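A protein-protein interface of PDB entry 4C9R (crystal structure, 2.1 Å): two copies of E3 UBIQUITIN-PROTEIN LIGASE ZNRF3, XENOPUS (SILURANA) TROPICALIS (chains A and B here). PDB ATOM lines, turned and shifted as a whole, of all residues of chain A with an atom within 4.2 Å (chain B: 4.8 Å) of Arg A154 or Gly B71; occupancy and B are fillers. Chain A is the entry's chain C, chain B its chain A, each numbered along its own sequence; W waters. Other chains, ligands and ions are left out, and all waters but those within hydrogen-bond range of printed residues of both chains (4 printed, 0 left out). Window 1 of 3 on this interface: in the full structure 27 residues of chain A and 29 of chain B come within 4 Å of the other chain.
Among the printed residues, merely in contact across the chains: Gly A48 with Arg B154 (3.5 Å), Arg A154 with Gly B48 (3.6 Å), Arg A154 with Tyr B70 (3.6 Å) and Arg A154 with Arg B154 (3.5 Å).
The guanidinium group (NE) of Arg B154 is in salt-bridge range of the side-chain carboxylate (OE2) of Glu B47 (2.8 Å).
The backbone NH of Gly B71 is in hydrogen-bond range of the backbone carbonyl oxygen of Gly B102 (2.8 Å).
The backbone NH (N) of Val A16 is in hydrogen-bond range of the backbone carbonyl oxygen (O) of Arg A154 (2.7 Å).
OE2 of Glu A47 is in salt-bridge range of NE of Arg A154.
OE2 of Glu A47 is in salt-bridge range of NE of Arg A156, at 3.2 Å.
O of Gly A48 sits at hydrogen-bond distance from N of Ala A155 (2.9 Å).
Water W4 lies within hydrogen-bond range of the guanidinium group of Arg A154 (2.9 Å) and the backbone carbonyl oxygen of Tyr B70 (3.3 Å).
Water W3 lies within hydrogen-bond range of N of Glu A49 (2.9 Å) and NH2 of Arg B154 (3.1 Å).
Water W2 bridges NH1 of Arg A156 (2.9 Å) and OH of Tyr B70 (3.3 Å).
Water W1 lies within hydrogen-bond range of N of Glu B49, O of Gly B71 and NH2 of Arg A154.
The backbone NH (N) of Glu A47 sits at hydrogen-bond distance from the side-chain carboxylate (OE1) of Glu B47, at 2.9 Å.
The backbone carbonyl oxygen (O) of Glu B47 lies within hydrogen-bond range of the guanidinium group (NH2) of Arg A154, at 2.8 Å.
The side-chain hydroxyl (OH) of Tyr B70 sits at hydrogen-bond distance from the guanidinium group (NH2) of Arg A156 (3.1 Å).
The guanidinium group of Arg A154 is in hydrogen-bond range of the backbone carbonyl oxygen of Gly B71 (3.1 Å).
The side-chain hydroxyl of Thr B104 is in hydrogen-bond range of the side-chain carboxylate of Glu A47 (2.7 Å).
The side-chain hydroxyl (OG1) of Thr B104 lies within hydrogen-bond range of the guanidinium group (NH2) of Arg A156, at 3.1 Å.
The guanidinium group of Arg B154 is in hydrogen-bond range of the backbone carbonyl oxygen of Glu A47.
Glu A49 touches none of the printed residues of chain B.
Of chain B, only Glu B47, Gly B48, Tyr B70, Gly B71 and Arg B154 come within 4 Å of Arg A154.
Trp B72 touches none of the printed residues of chain A.
Of the printed residues of chain A, Thr B104 touches Glu A47 and Arg A156.
Printed residues of chain A within 4 Å of Arg B154: Glu A47, Gly A48 and Arg A154.
The nearest residue of chain B that does not touch Arg A154 is Thr B104 (4.6 Å).
The nearest printed residue of chain A that does not touch Gly B71 is Glu A47 (4.8 Å).
Glu B47 touches its own counterpart, Glu A47.
Glu A47 touches Arg B154, and with the chains exchanged Arg A154 touches Glu B47.
Gly A48 touches Arg B154, and with the chains exchanged Arg A154 touches Gly B48.
Arg B154 touches its own counterpart, Arg A154.
4 positions are printed for both chains.
Of the 11 printed residues of chain A, 4 touch a printed residue of chain B.
Printed residues of chain B that touch a printed residue of chain A: Glu B47, Gly B48, Tyr B70, Gly B71, Thr B104 and Arg B154.
Hydrophobic or aromatic side chains of chain B within 4 Å of the printed part of chain A: Tyr B70.
Among the printed residues, 11 pairs touch across the chains.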
ATOM      1  N   GLU A  14     -15.006   3.165  -7.173  1.00  0.00           N
ATOM      2  CA  GLU A  14     -14.325   1.883  -7.231  1.00  0.00           C
ATOM      3  C   GLU A  14     -15.360   0.791  -7.045  1.00  0.00           C
ATOM      4  O   GLU A  14     -16.123   0.793  -6.083  1.00  0.00           O
ATOM      5  CB  GLU A  14     -13.286   1.779  -6.149  1.00  0.00           C
ATOM      6  CG  GLU A  14     -12.237   2.868  -6.222  1.00  0.00           C
ATOM      7  CD  GLU A  14     -11.375   2.954  -4.966  1.00  0.00           C
ATOM      8  OE1 GLU A  14     -11.302   1.954  -4.224  1.00  0.00           O
ATOM      9  OE2 GLU A  14     -10.782   4.037  -4.710  1.00  0.00           O
ATOM     10  N   VAL A  15     -15.432  -0.099  -7.995  1.00  0.00           N
ATOM     11  CA  VAL A  15     -16.274  -1.228  -7.832  1.00  0.00           C
ATOM     12  C   VAL A  15     -15.420  -2.434  -7.406  1.00  0.00           C
ATOM     13  O   VAL A  15     -14.470  -2.824  -8.098  1.00  0.00           O
ATOM     14  CB  VAL A  15     -17.062  -1.475  -9.096  1.00  0.00           C
ATOM     15  CG1 VAL A  15     -18.102  -2.555  -8.837  1.00  0.00           C
ATOM     16  CG2 VAL A  15     -17.694  -0.169  -9.550  1.00  0.00           C
ATOM     17  N   VAL A  16     -15.770  -3.029  -6.276  1.00  0.00           N
ATOM     18  CA  VAL A  16     -14.902  -4.019  -5.644  1.00  0.00           C
ATOM     19  C   VAL A  16     -15.614  -5.341  -5.736  1.00  0.00           C
ATOM     20  O   VAL A  16     -16.662  -5.501  -5.155  1.00  0.00           O
ATOM     21  CB  VAL A  16     -14.604  -3.684  -4.157  1.00  0.00           C
ATOM     22  CG1 VAL A  16     -13.577  -4.641  -3.516  1.00  0.00           C
ATOM     23  CG2 VAL A  16     -14.109  -2.246  -4.035  1.00  0.00           C
ATOM     24  N   GLU A  47     -19.928   4.399   0.796  1.00  0.00           N
ATOM     25  CA  GLU A  47     -19.566   3.055   0.403  1.00  0.00           C
ATOM     26  C   GLU A  47     -20.585   2.070   0.902  1.00  0.00           C
ATOM     27  O   GLU A  47     -21.155   2.229   1.994  1.00  0.00           O
ATOM     28  CB  GLU A  47     -18.146   2.753   0.908  1.00  0.00           C
ATOM     29  CG  GLU A  47     -17.846   1.298   1.153  1.00  0.00           C
ATOM     30  CD  GLU A  47     -16.459   1.059   1.759  1.00  0.00           C
ATOM     31  OE1 GLU A  47     -15.745   2.015   2.177  1.00  0.00           O
ATOM     32  OE2 GLU A  47     -16.092  -0.124   1.832  1.00  0.00           O
ATOM     33  N   GLY A  48     -20.860   1.055   0.101  1.00  0.00           N
ATOM     34  CA  GLY A  48     -21.727  -0.040   0.514  1.00  0.00           C
ATOM     35  C   GLY A  48     -21.938  -1.042  -0.601  1.00  0.00           C
ATOM     36  O   GLY A  48     -21.518  -0.829  -1.732  1.00  0.00           O
ATOM     37  N   GLU A  49     -22.645  -2.121  -0.271  1.00  0.00           N
ATOM     38  CA  GLU A  49     -22.979  -3.127  -1.230  1.00  0.00           C
ATOM     39  C   GLU A  49     -23.857  -2.588  -2.368  1.00  0.00           C
ATOM     40  O   GLU A  49     -24.771  -1.795  -2.160  1.00  0.00           O
ATOM     41  CB  GLU A  49     -23.623  -4.348  -0.579  1.00  0.00           C
ATOM     42  CG  GLU A  49     -24.859  -4.054   0.252  1.00  0.00           C
ATOM     43  CD  GLU A  49     -25.545  -5.326   0.774  1.00  0.00           C
ATOM     44  OE1 GLU A  49     -25.754  -6.272  -0.021  1.00  0.00           O
ATOM     45  OE2 GLU A  49     -25.881  -5.376   1.986  1.00  0.00           O
ATOM     46  N   ILE A  50     -23.568  -3.065  -3.570  1.00  0.00           N
ATOM     47  CA  ILE A  50     -24.273  -2.634  -4.751  1.00  0.00           C
ATOM     48  C   ILE A  50     -25.597  -3.393  -4.849  1.00  0.00           C
ATOM     49  O   ILE A  50     -25.623  -4.630  -4.720  1.00  0.00           O
ATOM     50  CB  ILE A  50     -23.449  -2.832  -6.050  1.00  0.00           C
ATOM     51  CG1 ILE A  50     -22.355  -1.789  -6.133  1.00  0.00           C
ATOM     52  CG2 ILE A  50     -24.341  -2.739  -7.273  1.00  0.00           C
ATOM     53  CD1 ILE A  50     -21.216  -2.116  -7.102  1.00  0.00           C
ATOM     54  N   ALA A 153     -20.918  -7.158  -5.337  1.00  0.00           N
ATOM     55  CA  ALA A 153     -19.858  -6.166  -5.499  1.00  0.00           C
ATOM     56  C   ALA A 153     -20.185  -5.068  -4.531  1.00  0.00           C
ATOM     57  O   ALA A 153     -21.349  -4.886  -4.148  1.00  0.00           O
ATOM     58  CB  ALA A 153     -19.810  -5.630  -6.913  1.00  0.00           C
ATOM     59  N   ARG A 154     -19.143  -4.381  -4.111  1.00  0.00           N
ATOM     60  CA  ARG A 154     -19.207  -3.265  -3.196  1.00  0.00           C
ATOM     61  C   ARG A 154     -18.788  -2.027  -3.967  1.00  0.00           C
ATOM     62  O   ARG A 154     -17.849  -2.080  -4.778  1.00  0.00           O
ATOM     63  CB  ARG A 154     -18.212  -3.485  -2.048  1.00  0.00           C
ATOM     64  CG  ARG A 154     -18.408  -2.524  -0.864  1.00  0.00           C
ATOM     65  CD  ARG A 154     -17.615  -2.917   0.377  1.00  0.00           C
ATOM     66  NE  ARG A 154     -17.972  -2.080   1.509  1.00  0.00           N
ATOM     67  CZ  ARG A 154     -19.032  -2.264   2.268  1.00  0.00           C
ATOM     68  NH1 ARG A 154     -19.822  -3.301   2.106  1.00  0.00           N
ATOM     69  NH2 ARG A 154     -19.292  -1.386   3.224  1.00  0.00           N
ATOM     70  N   ALA A 155     -19.471  -0.907  -3.751  1.00  0.00           N
ATOM     71  CA  ALA A 155     -19.042   0.345  -4.388  1.00  0.00           C
ATOM     72  C   ALA A 155     -18.382   1.219  -3.365  1.00  0.00           C
ATOM     73  O   ALA A 155     -18.889   1.350  -2.229  1.00  0.00           O
ATOM     74  CB  ALA A 155     -20.211   1.064  -5.049  1.00  0.00           C
ATOM     75  N   ARG A 156     -17.266   1.826  -3.753  1.00  0.00           N
ATOM     76  CA  ARG A 156     -16.631   2.896  -2.970  1.00  0.00           C
ATOM     77  C   ARG A 156     -16.603   4.157  -3.800  1.00  0.00           C
ATOM     78  O   ARG A 156     -15.805   4.268  -4.769  1.00  0.00           O
ATOM     79  CB  ARG A 156     -15.192   2.564  -2.571  1.00  0.00           C
ATOM     80  CG  ARG A 156     -15.100   1.439  -1.568  1.00  0.00           C
ATOM     81  CD  ARG A 156     -13.743   0.781  -1.487  1.00  0.00           C
ATOM     82  NE  ARG A 156     -13.778  -0.233  -0.435  1.00  0.00           N
ATOM     83  CZ  ARG A 156     -12.943  -1.270  -0.302  1.00  0.00           C
ATOM     84  NH1 ARG A 156     -11.991  -1.528  -1.218  1.00  0.00           N
ATOM     85  NH2 ARG A 156     -13.096  -2.076   0.752  1.00  0.00           N
ATOM     86  N   GLU B  47     -16.599   3.198   4.777  1.00  0.00           N
ATOM     87  CA  GLU B  47     -17.891   3.041   5.417  1.00  0.00           C
ATOM     88  C   GLU B  47     -18.296   1.592   5.423  1.00  0.00           C
ATOM     89  O   GLU B  47     -18.072   0.851   4.447  1.00  0.00           O
ATOM     90  CB  GLU B  47     -18.917   3.927   4.703  1.00  0.00           C
ATOM     91  CG  GLU B  47     -20.344   3.485   4.893  1.00  0.00           C
ATOM     92  CD  GLU B  47     -21.351   4.405   4.180  1.00  0.00           C
ATOM     93  OE1 GLU B  47     -20.945   5.241   3.355  1.00  0.00           O
ATOM     94  OE2 GLU B  47     -22.557   4.266   4.460  1.00  0.00           O
ATOM     95  N   GLY B  48     -18.935   1.170   6.503  1.00  0.00           N
ATOM     96  CA  GLY B  48     -19.353  -0.206   6.646  1.00  0.00           C
ATOM     97  C   GLY B  48     -19.968  -0.465   8.008  1.00  0.00           C
ATOM     98  O   GLY B  48     -19.882   0.338   8.950  1.00  0.00           O
ATOM     99  N   GLU B  49     -20.628  -1.582   8.110  1.00  0.00           N
ATOM    100  CA  GLU B  49     -21.205  -1.954   9.354  1.00  0.00           C
ATOM    101  C   GLU B  49     -20.169  -2.290  10.414  1.00  0.00           C
ATOM    102  O   GLU B  49     -19.111  -2.890  10.160  1.00  0.00           O
ATOM    103  CB  GLU B  49     -22.191  -3.118   9.205  1.00  0.00           C
ATOM    104  CG  GLU B  49     -21.656  -4.372   8.582  1.00  0.00           C
ATOM    105  CD  GLU B  49     -22.748  -5.444   8.521  1.00  0.00           C
ATOM    106  OE1 GLU B  49     -23.810  -5.213   7.845  1.00  0.00           O
ATOM    107  OE2 GLU B  49     -22.555  -6.497   9.173  1.00  0.00           O
ATOM    108  N   GLU B  69     -19.276 -11.021   6.239  1.00  0.00           N
ATOM    109  CA  GLU B  69     -19.628 -10.379   4.975  1.00  0.00           C
ATOM    110  C   GLU B  69     -18.532  -9.355   4.665  1.00  0.00           C
ATOM    111  O   GLU B  69     -18.137  -8.668   5.539  1.00  0.00           O
ATOM    112  CB  GLU B  69     -20.995  -9.670   5.119  1.00  0.00           C
ATOM    113  CG  GLU B  69     -22.029 -10.080   4.078  1.00  0.00           C
ATOM    114  CD  GLU B  69     -22.318 -11.584   4.083  1.00  0.00           C
ATOM    115  OE1 GLU B  69     -22.319 -12.200   5.179  1.00  0.00           O
ATOM    116  OE2 GLU B  69     -22.546 -12.160   2.984  1.00  0.00           O
ATOM    117  N   TYR B  70     -18.064  -9.250   3.438  1.00  0.00           N
ATOM    118  CA  TYR B  70     -17.028  -8.290   3.069  1.00  0.00           C
ATOM    119  C   TYR B  70     -17.431  -6.853   3.360  1.00  0.00           C
ATOM    120  O   TYR B  70     -18.571  -6.501   3.138  1.00  0.00           O
ATOM    121  CB  TYR B  70     -16.749  -8.364   1.565  1.00  0.00           C
ATOM    122  CG  TYR B  70     -15.581  -7.485   1.243  1.00  0.00           C
ATOM    123  CD1 TYR B  70     -14.290  -7.859   1.621  1.00  0.00           C
ATOM    124  CD2 TYR B  70     -15.746  -6.271   0.647  1.00  0.00           C
ATOM    125  CE1 TYR B  70     -13.216  -7.044   1.381  1.00  0.00           C
ATOM    126  CE2 TYR B  70     -14.680  -5.451   0.432  1.00  0.00           C
ATOM    127  CZ  TYR B  70     -13.418  -5.851   0.811  1.00  0.00           C
ATOM    128  OH  TYR B  70     -12.342  -5.038   0.609  1.00  0.00           O
ATOM    129  N   GLY B  71     -16.492  -6.031   3.832  1.00  0.00           N
ATOM    130  CA  GLY B  71     -16.660  -4.583   3.948  1.00  0.00           C
ATOM    131  C   GLY B  71     -17.098  -4.009   5.294  1.00  0.00           C
ATOM    132  O   GLY B  71     -17.702  -2.921   5.367  1.00  0.00           O
ATOM    133  N   TRP B  72     -16.782  -4.725   6.368  1.00  0.00           N
ATOM    134  CA  TRP B  72     -17.108  -4.290   7.739  1.00  0.00           C
ATOM    135  C   TRP B  72     -16.063  -3.344   8.307  1.00  0.00           C
ATOM    136  O   TRP B  72     -14.902  -3.352   7.885  1.00  0.00           O
ATOM    137  CB  TRP B  72     -17.287  -5.520   8.640  1.00  0.00           C
ATOM    138  CG  TRP B  72     -16.192  -6.627   8.566  1.00  0.00           C
ATOM    139  CD1 TRP B  72     -16.104  -7.628   7.670  1.00  0.00           C
ATOM    140  CD2 TRP B  72     -15.060  -6.798   9.454  1.00  0.00           C
ATOM    141  NE1 TRP B  72     -15.016  -8.443   7.948  1.00  0.00           N
ATOM    142  CE2 TRP B  72     -14.350  -7.936   9.023  1.00  0.00           C
ATOM    143  CE3 TRP B  72     -14.610  -6.117  10.589  1.00  0.00           C
ATOM    144  CZ2 TRP B  72     -13.216  -8.402   9.676  1.00  0.00           C
ATOM    145  CZ3 TRP B  72     -13.484  -6.574  11.229  1.00  0.00           C
ATOM    146  CH2 TRP B  72     -12.803  -7.721  10.785  1.00  0.00           C
ATOM    147  N   VAL B  73     -16.483  -2.464   9.230  1.00  0.00           N
ATOM    148  CA  VAL B  73     -15.555  -1.650   9.949  1.00  0.00           C
ATOM    149  C   VAL B  73     -15.284  -2.288  11.301  1.00  0.00           C
ATOM    150  O   VAL B  73     -16.184  -2.375  12.127  1.00  0.00           O
ATOM    151  CB  VAL B  73     -16.099  -0.228  10.159  1.00  0.00           C
ATOM    152  CG1 VAL B  73     -15.248   0.632  11.089  1.00  0.00           C
ATOM    153  CG2 VAL B  73     -16.228   0.437   8.810  1.00  0.00           C
ATOM    154  N   GLY B 102     -11.760  -9.164   5.602  1.00  0.00           N
ATOM    155  CA  GLY B 102     -12.756  -8.420   4.900  1.00  0.00           C
ATOM    156  C   GLY B 102     -13.054  -7.035   5.472  1.00  0.00           C
ATOM    157  O   GLY B 102     -13.984  -6.387   5.002  1.00  0.00           O
ATOM    158  N   THR B 104     -13.183  -3.189   5.865  1.00  0.00           N
ATOM    159  CA  THR B 104     -12.995  -2.042   5.020  1.00  0.00           C
ATOM    160  C   THR B 104     -12.192  -0.951   5.724  1.00  0.00           C
ATOM    161  O   THR B 104     -11.647  -0.067   5.096  1.00  0.00           O
ATOM    162  CB  THR B 104     -14.313  -1.492   4.436  1.00  0.00           C
ATOM    163  OG1 THR B 104     -13.962  -0.685   3.331  1.00  0.00           O
ATOM    164  CG2 THR B 104     -15.091  -0.632   5.470  1.00  0.00           C
ATOM    165  N   ARG B 154     -23.605   1.659  11.676  1.00  0.00           N
ATOM    166  CA  ARG B 154     -22.778   1.792  10.469  1.00  0.00           C
ATOM    167  C   ARG B 154     -21.842   2.933  10.760  1.00  0.00           C
ATOM    168  O   ARG B 154     -22.271   3.971  11.254  1.00  0.00           O
ATOM    169  CB  ARG B 154     -23.643   2.133   9.224  1.00  0.00           C
ATOM    170  CG  ARG B 154     -22.949   1.887   7.886  1.00  0.00           C
ATOM    171  CD  ARG B 154     -23.905   2.012   6.735  1.00  0.00           C
ATOM    172  NE  ARG B 154     -23.209   1.782   5.500  1.00  0.00           N
ATOM    173  CZ  ARG B 154     -22.881   0.582   5.075  1.00  0.00           C
ATOM    174  NH1 ARG B 154     -23.227  -0.501   5.769  1.00  0.00           N
ATOM    175  NH2 ARG B 154     -22.189   0.476   3.964  1.00  0.00           N
HETATM  176  O   HOH W   1     -20.848  -3.100   5.611  1.00  0.00           O
HETATM  177  O   HOH W   2      -9.933  -3.564  -1.144  1.00  0.00           O
HETATM  178  O   HOH W   3     -23.265  -2.097   2.550  1.00  0.00           O
HETATM  179  O   HOH W   4     -19.594  -5.415   0.156  1.00  0.00           O
